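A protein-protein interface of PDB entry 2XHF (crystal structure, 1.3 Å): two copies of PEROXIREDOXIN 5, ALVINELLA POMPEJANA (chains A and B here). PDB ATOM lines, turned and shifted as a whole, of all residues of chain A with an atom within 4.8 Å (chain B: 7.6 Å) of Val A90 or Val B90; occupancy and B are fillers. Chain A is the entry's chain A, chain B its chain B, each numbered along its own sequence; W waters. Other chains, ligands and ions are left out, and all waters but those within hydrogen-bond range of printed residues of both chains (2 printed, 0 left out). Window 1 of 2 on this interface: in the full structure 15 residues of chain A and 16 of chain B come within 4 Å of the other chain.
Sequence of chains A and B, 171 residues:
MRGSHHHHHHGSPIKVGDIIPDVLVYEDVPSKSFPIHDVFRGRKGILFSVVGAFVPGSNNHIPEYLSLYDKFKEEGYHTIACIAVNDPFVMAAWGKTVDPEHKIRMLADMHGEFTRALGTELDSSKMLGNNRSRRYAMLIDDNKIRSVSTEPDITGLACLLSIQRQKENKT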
ATOM      1  N   ALA A  53      16.421 -18.877 -14.799  1.00  0.00           N
ATOM      2  CA  ALA A  53      15.377 -17.907 -14.507  1.00  0.00           C
ATOM      3  C   ALA A  53      14.446 -17.855 -15.729  1.00  0.00           C
ATOM      4  O   ALA A  53      14.907 -17.791 -16.881  1.00  0.00           O
ATOM      5  CB  ALA A  53      16.002 -16.569 -14.275  1.00  0.00           C
ATOM      6  N   PHE A  54      13.135 -17.879 -15.462  1.00  0.00           N
ATOM      7  CA  PHE A  54      12.084 -17.760 -16.487  1.00  0.00           C
ATOM      8  C   PHE A  54      11.968 -18.965 -17.429  1.00  0.00           C
ATOM      9  O   PHE A  54      11.135 -18.968 -18.323  1.00  0.00           O
ATOM     10  CB  PHE A  54      12.246 -16.462 -17.294  1.00  0.00           C
ATOM     11  CG  PHE A  54      12.093 -15.221 -16.459  1.00  0.00           C
ATOM     12  CD1 PHE A  54      10.849 -14.831 -15.995  1.00  0.00           C
ATOM     13  CD2 PHE A  54      13.192 -14.448 -16.137  1.00  0.00           C
ATOM     14  CE1 PHE A  54      10.714 -13.696 -15.215  1.00  0.00           C
ATOM     15  CE2 PHE A  54      13.054 -13.301 -15.378  1.00  0.00           C
ATOM     16  CZ  PHE A  54      11.822 -12.932 -14.924  1.00  0.00           C
ATOM     17  N   ASN A  86      22.889 -17.972 -14.701  1.00  0.00           N
ATOM     18  CA  ASN A  86      22.281 -16.732 -15.196  1.00  0.00           C
ATOM     19  C   ASN A  86      23.120 -15.594 -14.663  1.00  0.00           C
ATOM     20  O   ASN A  86      23.848 -15.757 -13.668  1.00  0.00           O
ATOM     21  CB  ASN A  86      20.865 -16.528 -14.669  1.00  0.00           C
ATOM     22  CG  ASN A  86      19.810 -17.253 -15.482  1.00  0.00           C
ATOM     23  OD1 ASN A  86      19.213 -18.201 -15.009  1.00  0.00           O
ATOM     24  ND2 ASN A  86      19.567 -16.798 -16.712  1.00  0.00           N
ATOM     25  N   ASP A  87      22.981 -14.428 -15.272  1.00  0.00           N
ATOM     26  CA  ASP A  87      23.547 -13.221 -14.693  1.00  0.00           C
ATOM     27  C   ASP A  87      22.669 -12.790 -13.511  1.00  0.00           C
ATOM     28  O   ASP A  87      21.484 -13.129 -13.448  1.00  0.00           O
ATOM     29  CB  ASP A  87      23.727 -12.112 -15.749  1.00  0.00           C
ATOM     30  CG  ASP A  87      22.420 -11.443 -16.150  1.00  0.00           C
ATOM     31  OD1 ASP A  87      21.981 -11.594 -17.328  1.00  0.00           O
ATOM     32  OD2 ASP A  87      21.826 -10.747 -15.294  1.00  0.00           O
ATOM     33  N   PRO A  88      23.248 -12.043 -12.556  1.00  0.00           N
ATOM     34  CA  PRO A  88      22.489 -11.721 -11.348  1.00  0.00           C
ATOM     35  C   PRO A  88      21.359 -10.727 -11.532  1.00  0.00           C
ATOM     36  O   PRO A  88      20.436 -10.749 -10.745  1.00  0.00           O
ATOM     37  CB  PRO A  88      23.554 -11.164 -10.401  1.00  0.00           C
ATOM     38  CG  PRO A  88      24.639 -10.694 -11.305  1.00  0.00           C
ATOM     39  CD  PRO A  88      24.660 -11.649 -12.452  1.00  0.00           C
ATOM     40  N   PHE A  89      21.388  -9.893 -12.569  1.00  0.00           N
ATOM     41  CA  PHE A  89      20.247  -8.986 -12.796  1.00  0.00           C
ATOM     42  C   PHE A  89      19.006  -9.810 -13.136  1.00  0.00           C
ATOM     43  O   PHE A  89      17.913  -9.612 -12.580  1.00  0.00           O
ATOM     44  CB  PHE A  89      20.530  -7.998 -13.913  1.00  0.00           C
ATOM     45  CG  PHE A  89      21.664  -7.049 -13.638  1.00  0.00           C
ATOM     46  CD1 PHE A  89      21.614  -6.168 -12.561  1.00  0.00           C
ATOM     47  CD2 PHE A  89      22.773  -7.011 -14.472  1.00  0.00           C
ATOM     48  CE1 PHE A  89      22.633  -5.241 -12.364  1.00  0.00           C
ATOM     49  CE2 PHE A  89      23.784  -6.075 -14.283  1.00  0.00           C
ATOM     50  CZ  PHE A  89      23.715  -5.218 -13.198  1.00  0.00           C
ATOM     51  N   VAL A  90      19.182 -10.757 -14.048  1.00  0.00           N
ATOM     52  CA  VAL A  90      18.090 -11.608 -14.453  1.00  0.00           C
ATOM     53  C   VAL A  90      17.652 -12.469 -13.266  1.00  0.00           C
ATOM     54  O   VAL A  90      16.474 -12.620 -12.981  1.00  0.00           O
ATOM     55  CB  VAL A  90      18.493 -12.477 -15.656  1.00  0.00           C
ATOM     56  CG1 VAL A  90      17.470 -13.571 -15.847  1.00  0.00           C
ATOM     57  CG2 VAL A  90      18.645 -11.616 -16.914  1.00  0.00           C
ATOM     58  N   MET A  91      18.616 -13.049 -12.566  1.00  0.00           N
ATOM     59  CA  MET A  91      18.282 -13.939 -11.453  1.00  0.00           C
ATOM     60  C   MET A  91      17.496 -13.208 -10.364  1.00  0.00           C
ATOM     61  O   MET A  91      16.506 -13.707  -9.879  1.00  0.00           O
ATOM     62  CB  MET A  91      19.556 -14.540 -10.874  1.00  0.00           C
ATOM     63  CG  MET A  91      19.262 -15.612  -9.910  1.00  0.00           C
ATOM     64  SD  MET A  91      18.807 -17.117 -10.754  1.00  0.00           S
ATOM     65  CE  MET A  91      18.767 -18.273  -9.336  1.00  0.00           C
ATOM     66  N   ALA A  92      17.929 -12.002 -10.014  1.00  0.00           N
ATOM     67  CA  ALA A  92      17.272 -11.250  -8.956  1.00  0.00           C
ATOM     68  C   ALA A  92      15.856 -10.843  -9.362  1.00  0.00           C
ATOM     69  O   ALA A  92      14.938 -10.895  -8.552  1.00  0.00           O
ATOM     70  CB  ALA A  92      18.101 -10.021  -8.578  1.00  0.00           C
ATOM     71  N   ALA A  93      15.682 -10.416 -10.616  1.00  0.00           N
ATOM     72  CA  ALA A  93      14.372  -9.973 -11.089  1.00  0.00           C
ATOM     73  C   ALA A  93      13.432 -11.164 -11.044  1.00  0.00           C
ATOM     74  O   ALA A  93      12.301 -11.066 -10.619  1.00  0.00           O
ATOM     75  CB  ALA A  93      14.457  -9.415 -12.488  1.00  0.00           C
ATOM     76  N   TRP A  94      13.923 -12.299 -11.514  1.00  0.00           N
ATOM     77  CA  TRP A  94      13.130 -13.518 -11.487  1.00  0.00           C
ATOM     78  C   TRP A  94      12.727 -13.918 -10.062  1.00  0.00           C
ATOM     79  O   TRP A  94      11.568 -14.243  -9.778  1.00  0.00           O
ATOM     80  CB  TRP A  94      13.893 -14.655 -12.153  1.00  0.00           C
ATOM     81  CG  TRP A  94      13.169 -15.964 -12.106  1.00  0.00           C
ATOM     82  CD1 TRP A  94      12.023 -16.281 -12.752  1.00  0.00           C
ATOM     83  CD2 TRP A  94      13.535 -17.106 -11.349  1.00  0.00           C
ATOM     84  NE1 TRP A  94      11.660 -17.582 -12.483  1.00  0.00           N
ATOM     85  CE2 TRP A  94      12.564 -18.098 -11.591  1.00  0.00           C
ATOM     86  CE3 TRP A  94      14.595 -17.398 -10.488  1.00  0.00           C
ATOM     87  CZ2 TRP A  94      12.627 -19.353 -11.022  1.00  0.00           C
ATOM     88  CZ3 TRP A  94      14.645 -18.645  -9.908  1.00  0.00           C
ATOM     89  CH2 TRP A  94      13.672 -19.620 -10.192  1.00  0.00           C
ATOM     90  N   ASP B  28      10.284 -15.495 -28.022  1.00  0.00           N
ATOM     91  CA  ASP B  28       9.372 -16.223 -27.098  1.00  0.00           C
ATOM     92  C   ASP B  28       9.927 -17.547 -26.546  1.00  0.00           C
ATOM     93  O   ASP B  28      10.047 -17.710 -25.318  1.00  0.00           O
ATOM     94  CB  ASP B  28       7.968 -16.429 -27.712  1.00  0.00           C
ATOM     95  CG  ASP B  28       7.279 -15.124 -27.995  1.00  0.00           C
ATOM     96  OD1 ASP B  28       7.120 -14.308 -27.049  1.00  0.00           O
ATOM     97  OD2 ASP B  28       6.932 -14.895 -29.169  1.00  0.00           O
ATOM     98  N   GLY B  52      21.229  -6.250 -22.032  1.00  0.00           N
ATOM     99  CA  GLY B  52      20.549  -7.464 -21.649  1.00  0.00           C
ATOM    100  C   GLY B  52      19.227  -7.162 -21.002  1.00  0.00           C
ATOM    101  O   GLY B  52      19.043  -6.082 -20.435  1.00  0.00           O
ATOM    102  N   ALA B  53      18.335  -8.142 -21.052  1.00  0.00           N
ATOM    103  CA  ALA B  53      17.111  -8.098 -20.284  1.00  0.00           C
ATOM    104  C   ALA B  53      17.450  -7.860 -18.820  1.00  0.00           C
ATOM    105  O   ALA B  53      18.343  -8.507 -18.274  1.00  0.00           O
ATOM    106  CB  ALA B  53      16.367  -9.418 -20.454  1.00  0.00           C
ATOM    107  N   PHE B  54      16.757  -6.908 -18.194  1.00  0.00           N
ATOM    108  CA  PHE B  54      16.890  -6.618 -16.758  1.00  0.00           C
ATOM    109  C   PHE B  54      18.209  -5.919 -16.397  1.00  0.00           C
ATOM    110  O   PHE B  54      18.446  -5.623 -15.236  1.00  0.00           O
ATOM    111  CB  PHE B  54      16.668  -7.882 -15.895  1.00  0.00           C
ATOM    112  CG  PHE B  54      15.272  -8.439 -15.999  1.00  0.00           C
ATOM    113  CD1 PHE B  54      14.217  -7.794 -15.403  1.00  0.00           C
ATOM    114  CD2 PHE B  54      15.030  -9.602 -16.715  1.00  0.00           C
ATOM    115  CE1 PHE B  54      12.919  -8.309 -15.520  1.00  0.00           C
ATOM    116  CE2 PHE B  54      13.753 -10.113 -16.837  1.00  0.00           C
ATOM    117  CZ  PHE B  54      12.688  -9.460 -16.246  1.00  0.00           C
ATOM    118  N   VAL B  55      19.070  -5.654 -17.365  1.00  0.00           N
ATOM    119  CA  VAL B  55      20.316  -4.951 -17.068  1.00  0.00           C
ATOM    120  C   VAL B  55      20.011  -3.467 -16.891  1.00  0.00           C
ATOM    121  O   VAL B  55      19.283  -2.895 -17.681  1.00  0.00           O
ATOM    122  CB  VAL B  55      21.341  -5.154 -18.186  1.00  0.00           C
ATOM    123  CG1 VAL B  55      22.587  -4.305 -17.958  1.00  0.00           C
ATOM    124  CG2 VAL B  55      21.687  -6.625 -18.321  1.00  0.00           C
ATOM    125  N   VAL B  85      21.396 -10.172 -26.413  1.00  0.00           N
ATOM    126  CA  VAL B  85      21.995 -11.483 -26.269  1.00  0.00           C
ATOM    127  C   VAL B  85      21.479 -12.076 -24.953  1.00  0.00           C
ATOM    128  O   VAL B  85      22.029 -11.833 -23.869  1.00  0.00           O
ATOM    129  CB  VAL B  85      23.531 -11.396 -26.314  1.00  0.00           C
ATOM    130  CG1 VAL B  85      24.119 -12.768 -26.183  1.00  0.00           C
ATOM    131  CG2 VAL B  85      23.987 -10.748 -27.624  1.00  0.00           C
ATOM    132  N   ASN B  86      20.370 -12.809 -25.075  1.00  0.00           N
ATOM    133  CA  ASN B  86      19.660 -13.468 -23.989  1.00  0.00           C
ATOM    134  C   ASN B  86      18.946 -14.672 -24.597  1.00  0.00           C
ATOM    135  O   ASN B  86      18.676 -14.706 -25.812  1.00  0.00           O
ATOM    136  CB  ASN B  86      18.591 -12.565 -23.358  1.00  0.00           C
ATOM    137  CG  ASN B  86      19.142 -11.608 -22.328  1.00  0.00           C
ATOM    138  OD1 ASN B  86      19.187 -10.394 -22.548  1.00  0.00           O
ATOM    139  ND2 ASN B  86      19.547 -12.140 -21.174  1.00  0.00           N
ATOM    140  N   ASP B  87      18.587 -15.647 -23.775  1.00  0.00           N
ATOM    141  CA  ASP B  87      17.674 -16.721 -24.178  1.00  0.00           C
ATOM    142  C   ASP B  87      16.254 -16.144 -24.325  1.00  0.00           C
ATOM    143  O   ASP B  87      15.926 -15.090 -23.759  1.00  0.00           O
ATOM    144  CB  ASP B  87      17.748 -17.913 -23.217  1.00  0.00           C
ATOM    145  CG  ASP B  87      17.026 -17.672 -21.890  1.00  0.00           C
ATOM    146  OD1 ASP B  87      15.773 -17.580 -21.909  1.00  0.00           O
ATOM    147  OD2 ASP B  87      17.716 -17.635 -20.840  1.00  0.00           O
ATOM    148  N   PRO B  88      15.420 -16.787 -25.154  1.00  0.00           N
ATOM    149  CA  PRO B  88      14.133 -16.173 -25.457  1.00  0.00           C
ATOM    150  C   PRO B  88      13.150 -16.201 -24.309  1.00  0.00           C
ATOM    151  O   PRO B  88      12.243 -15.353 -24.277  1.00  0.00           O
ATOM    152  CB  PRO B  88      13.635 -16.971 -26.674  1.00  0.00           C
ATOM    153  CG  PRO B  88      14.383 -18.243 -26.627  1.00  0.00           C
ATOM    154  CD  PRO B  88      15.720 -17.913 -26.044  1.00  0.00           C
ATOM    155  N   PHE B  89      13.287 -17.124 -23.367  1.00  0.00           N
ATOM    156  CA  PHE B  89      12.371 -17.110 -22.237  1.00  0.00           C
ATOM    157  C   PHE B  89      12.579 -15.839 -21.415  1.00  0.00           C
ATOM    158  O   PHE B  89      11.627 -15.154 -21.027  1.00  0.00           O
ATOM    159  CB  PHE B  89      12.588 -18.329 -21.347  1.00  0.00           C
ATOM    160  CG  PHE B  89      12.233 -19.651 -21.993  1.00  0.00           C
ATOM    161  CD1 PHE B  89      10.928 -19.913 -22.425  1.00  0.00           C
ATOM    162  CD2 PHE B  89      13.189 -20.632 -22.150  1.00  0.00           C
ATOM    163  CE1 PHE B  89      10.607 -21.156 -22.990  1.00  0.00           C
ATOM    164  CE2 PHE B  89      12.871 -21.875 -22.708  1.00  0.00           C
ATOM    165  CZ  PHE B  89      11.583 -22.128 -23.132  1.00  0.00           C
ATOM    166  N   VAL B  90      13.843 -15.534 -21.152  1.00  0.00           N
ATOM    167  CA  VAL B  90      14.168 -14.337 -20.379  1.00  0.00           C
ATOM    168  C   VAL B  90      13.774 -13.089 -21.190  1.00  0.00           C
ATOM    169  O   VAL B  90      13.169 -12.139 -20.667  1.00  0.00           O
ATOM    170  CB  VAL B  90      15.666 -14.313 -20.038  1.00  0.00           C
ATOM    171  CG1 VAL B  90      16.086 -12.935 -19.528  1.00  0.00           C
ATOM    172  CG2 VAL B  90      15.989 -15.373 -19.031  1.00  0.00           C
ATOM    173  N   MET B  91      14.093 -13.077 -22.481  1.00  0.00           N
ATOM    174  CA  MET B  91      13.789 -11.906 -23.292  1.00  0.00           C
ATOM    175  C   MET B  91      12.286 -11.612 -23.331  1.00  0.00           C
ATOM    176  O   MET B  91      11.873 -10.460 -23.168  1.00  0.00           O
ATOM    177  CB  MET B  91      14.338 -12.098 -24.705  1.00  0.00           C
ATOM    178  CG  MET B  91      14.304 -10.870 -25.520  1.00  0.00           C
ATOM    179  SD  MET B  91      15.580  -9.719 -24.984  1.00  0.00           S
ATOM    180  CE  MET B  91      15.326  -8.401 -26.207  1.00  0.00           C
ATOM    181  N   ALA B  92      11.472 -12.651 -23.513  1.00  0.00           N
ATOM    182  CA  ALA B  92      10.031 -12.472 -23.611  1.00  0.00           C
ATOM    183  C   ALA B  92       9.456 -12.013 -22.276  1.00  0.00           C
ATOM    184  O   ALA B  92       8.573 -11.161 -22.228  1.00  0.00           O
ATOM    185  CB  ALA B  92       9.366 -13.768 -24.047  1.00  0.00           C
ATOM    186  N   ALA B  93       9.946 -12.570 -21.169  1.00  0.00           N
ATOM    187  CA  ALA B  93       9.409 -12.219 -19.856  1.00  0.00           C
ATOM    188  C   ALA B  93       9.750 -10.760 -19.580  1.00  0.00           C
ATOM    189  O   ALA B  93       8.935  -9.993 -19.092  1.00  0.00           O
ATOM    190  CB  ALA B  93       9.996 -13.097 -18.789  1.00  0.00           C
ATOM    191  N   TRP B  94      10.982 -10.384 -19.881  1.00  0.00           N
ATOM    192  CA  TRP B  94      11.407  -9.010 -19.719  1.00  0.00           C
ATOM    193  C   TRP B  94      10.555  -8.070 -20.573  1.00  0.00           C
ATOM    194  O   TRP B  94      10.102  -7.010 -20.115  1.00  0.00           O
ATOM    195  CB  TRP B  94      12.881  -8.859 -20.084  1.00  0.00           C
ATOM    196  CG  TRP B  94      13.359  -7.437 -19.992  1.00  0.00           C
ATOM    197  CD1 TRP B  94      13.494  -6.690 -18.861  1.00  0.00           C
ATOM    198  CD2 TRP B  94      13.739  -6.601 -21.079  1.00  0.00           C
ATOM    199  NE1 TRP B  94      13.957  -5.439 -19.174  1.00  0.00           N
ATOM    200  CE2 TRP B  94      14.104  -5.356 -20.539  1.00  0.00           C
ATOM    201  CE3 TRP B  94      13.791  -6.777 -22.462  1.00  0.00           C
ATOM    202  CZ2 TRP B  94      14.516  -4.294 -21.328  1.00  0.00           C
ATOM    203  CZ3 TRP B  94      14.220  -5.735 -23.238  1.00  0.00           C
ATOM    204  CH2 TRP B  94      14.563  -4.499 -22.686  1.00  0.00           C
ATOM    205  N   GLY B  95      10.357  -8.449 -21.824  1.00  0.00           N
ATOM    206  CA  GLY B  95       9.570  -7.643 -22.741  1.00  0.00           C
ATOM    207  C   GLY B  95       8.194  -7.331 -22.177  1.00  0.00           C
ATOM    208  O   GLY B  95       7.703  -6.216 -22.292  1.00  0.00           O
ATOM    209  N   LYS B  96       7.557  -8.328 -21.576  1.00  0.00           N
ATOM    210  CA  LYS B  96       6.239  -8.128 -21.007  1.00  0.00           C
ATOM    211  C   LYS B  96       6.264  -7.116 -19.860  1.00  0.00           C
ATOM    212  O   LYS B  96       5.274  -6.440 -19.629  1.00  0.00           O
ATOM    213  CB  LYS B  96       5.644  -9.452 -20.538  1.00  0.00           C
ATOM    214  CG  LYS B  96       5.245 -10.352 -21.686  1.00  0.00           C
ATOM    215  CD  LYS B  96       4.626 -11.644 -21.163  1.00  0.00           C
ATOM    216  CE  LYS B  96       4.158 -12.542 -22.300  1.00  0.00           C
ATOM    217  NZ  LYS B  96       5.269 -13.327 -22.918  1.00  0.00           N
ATOM    218  N   THR B  97       7.376  -7.022 -19.125  1.00  0.00           N
ATOM    219  CA  THR B  97       7.444  -6.052 -18.029  1.00  0.00           C
ATOM    220  C   THR B  97       7.670  -4.620 -18.507  1.00  0.00           C
ATOM    221  O   THR B  97       7.212  -3.673 -17.874  1.00  0.00           O
ATOM    222  CB  THR B  97       8.528  -6.385 -16.998  1.00  0.00           C
ATOM    223  OG1 THR B  97       9.821  -6.075 -17.543  1.00  0.00           O
ATOM    224  CG2 THR B  97       8.457  -7.851 -16.576  1.00  0.00           C
ATOM    225  N   MET B 106      10.542  -8.492 -29.467  1.00  0.00           N
ATOM    226  CA  MET B 106      11.638  -8.780 -28.558  1.00  0.00           C
ATOM    227  C   MET B 106      12.440  -9.944 -29.110  1.00  0.00           C
ATOM    228  O   MET B 106      12.029 -11.097 -29.046  1.00  0.00           O
ATOM    229  CB  MET B 106      11.087  -9.112 -27.166  1.00  0.00           C
ATOM    230  CG  MET B 106      10.431  -7.912 -26.511  1.00  0.00           C
ATOM    231  SD  MET B 106      11.700  -6.854 -25.777  1.00  0.00           S
ATOM    232  CE  MET B 106      10.816  -5.304 -25.564  1.00  0.00           C
ATOM    233  N   ALA B 108      15.705 -12.335 -29.413  1.00  0.00           N
ATOM    234  CA  ALA B 108      16.749 -12.925 -28.584  1.00  0.00           C
ATOM    235  C   ALA B 108      17.857 -13.444 -29.489  1.00  0.00           C
ATOM    236  O   ALA B 108      17.688 -14.426 -30.209  1.00  0.00           O
ATOM    237  CB  ALA B 108      16.186 -14.048 -27.702  1.00  0.00           C
ATOM    238  N   LEU B 128      29.019 -10.087 -16.977  1.00  0.00           N
ATOM    239  CA  LEU B 128      27.738 -10.698 -17.278  1.00  0.00           C
ATOM    240  C   LEU B 128      27.809 -12.134 -17.750  1.00  0.00           C
ATOM    241  O   LEU B 128      26.784 -12.699 -18.134  1.00  0.00           O
ATOM    242  CB  LEU B 128      27.021  -9.869 -18.338  1.00  0.00           C
ATOM    243  CG  LEU B 128      26.594  -8.466 -17.904  1.00  0.00           C
ATOM    244  CD1 LEU B 128      26.060  -7.679 -19.104  1.00  0.00           C
ATOM    245  CD2 LEU B 128      25.547  -8.514 -16.801  1.00  0.00           C
ATOM    246  N   ARG B 132      27.922  -9.462 -24.628  1.00  0.00           N
ATOM    247  CA  ARG B 132      26.628  -8.909 -24.959  1.00  0.00           C
ATOM    248  C   ARG B 132      26.803  -7.925 -26.115  1.00  0.00           C
ATOM    249  O   ARG B 132      27.862  -7.769 -26.670  1.00  0.00           O
ATOM    250  CB  ARG B 132      25.987  -8.217 -23.740  1.00  0.00           C
ATOM    251  CG  ARG B 132      25.749  -9.105 -22.518  1.00  0.00           C
ATOM    252  CD  ARG B 132      24.842 -10.305 -22.825  1.00  0.00           C
ATOM    253  NE  ARG B 132      24.669 -11.151 -21.642  1.00  0.00           N
ATOM    254  CZ  ARG B 132      23.747 -10.951 -20.711  1.00  0.00           C
ATOM    255  NH1 ARG B 132      22.869  -9.953 -20.831  1.00  0.00           N
ATOM    256  NH2 ARG B 132      23.662 -11.774 -19.673  1.00  0.00           N
HETATM  257  O   HOH W   1      20.574 -10.092 -19.168  1.00  0.00           O
HETATM  258  O   HOH W   2      17.340 -18.281 -18.182  1.00  0.00           O
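The side-chain carboxylate (OD1) of Asp A87 lies within salt-bridge range of the guanidinium group (NH2) of Arg B132 (2.9 Å).
The backbone NH (N) of Phe B89 is in hydrogen-bond range of the side-chain carboxylate (OD1) of Asp B87 (2.9 Å).
The side-chain carboxylate of Asp A87 lies within hydrogen-bond range of the backbone NH of Val A90 (2.9 Å).
The backbone NH (N) of Val B90 sits at hydrogen-bond distance from the side-chain carboxylate (OD1) of Asp B87 (2.9 Å).
N of Ala B53 sits at hydrogen-bond distance from OD1 of Asn B86 (2.8 Å).
The side-chain amide oxygen (OD1) of Asn A86 is in hydrogen-bond range of the backbone NH (N) of Ala A53 (2.9 Å).
The side-chain carboxylate (OD2) of Asp A87 is in hydrogen-bond range of the backbone NH (N) of Phe A89, 2.9 Å away.
Ala A53 touches Val B90 (O to CG2, 3.4 Å).
Phe A54 touches Phe B54.
CB of Phe B89 touches O of Phe A54, 3.4 Å away.
CB of Ala B93 touches CD1 of Phe A54, at 3.4 Å.
O of Leu B128 touches CB of Asp A87 (3.9 Å).
Phe A89 touches Phe B54 (CB to O, 3.4 Å).
Leu B128 touches Phe A89 (CD2 to CD2, 3.9 Å).
Val A90 touches Ala B53.
Val A90 touches Val B90 (CG2 to CG1, 3.9 Å).
Ala A93 touches Phe B54 (CB to CD1, 3.3 Å).
Printed residues of chain B within 4 Å of Ala A53: Val B90.
Printed residues of chain B within 4 Å of Phe A54: Phe B54 (3.6 Å), Phe B89 (3.4 Å) and Ala B93 (3.4 Å).
Of chain B, only Ala B53 (3.4 Å) and Val B90 (3.9 Å) come within 4 Å of Val A90.
Pro B88 touches none of the printed residues of chain A.
Of chain A, only Ala A53 and Val A90 come within 4 Å of Val B90.
Of the printed residues of chain A, Ala B93 touches Phe A54.
The nearest residue of chain B that does not touch Val A90 is Phe B54 (4.1 Å).
The nearest printed residue of chain A that does not touch Ala B93 is Ala A53 (7.1 Å).
Printed residues of chain A that touch a printed residue of chain B: Ala A53, Phe A54, Asp A87, Phe A89, Val A90 and Ala A93.
Hydrophobic or aromatic side chains of chain A that line the printed part of chain B: Phe A54, Phe A89, Val A90 and Ala A93.
Hydrophobic or aromatic side chains of chain B within 4 Å of the printed part of chain A: Phe B54, Phe B89, Val B90, Ala B93 and Leu B128.
Among the printed residues, 11 pairs touch across the chains.
Among the printed residues, Asp or Glu carboxylates within 4 Å of a Lys or Arg side-chain nitrogen of the other chain: Asp A87 with Arg B132 (2.9 Å).
Ala A53 touches Val B90, and with the chains exchanged Val A90 touches Ala B53.
Phe A54 touches Phe B89, and with the chains exchanged Phe A89 touches Phe B54.
Phe A54 touches Ala B93, and with the chains exchanged Ala A93 touches Phe B54.
Val A90 touches its own counterpart, Val B90.
Of the 11 pairs that touch across the chains among the printed residues, 8 have their exchanged pair printed and touching as well.
Water W1 lies within hydrogen-bond range of the side-chain carboxylate of Asp A87 (2.8 Å), the guanidinium group of Arg B132 (2.8 Å), the backbone carbonyl oxygen of Ala B53 (2.9 Å) and the side-chain amide nitrogen of Asn B86 (3.0 Å).
Water W2 lies within hydrogen-bond range of the side-chain carboxylate of Asp B87, the backbone carbonyl oxygen of Ala A53 and the side-chain amide nitrogen of Asn A86.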
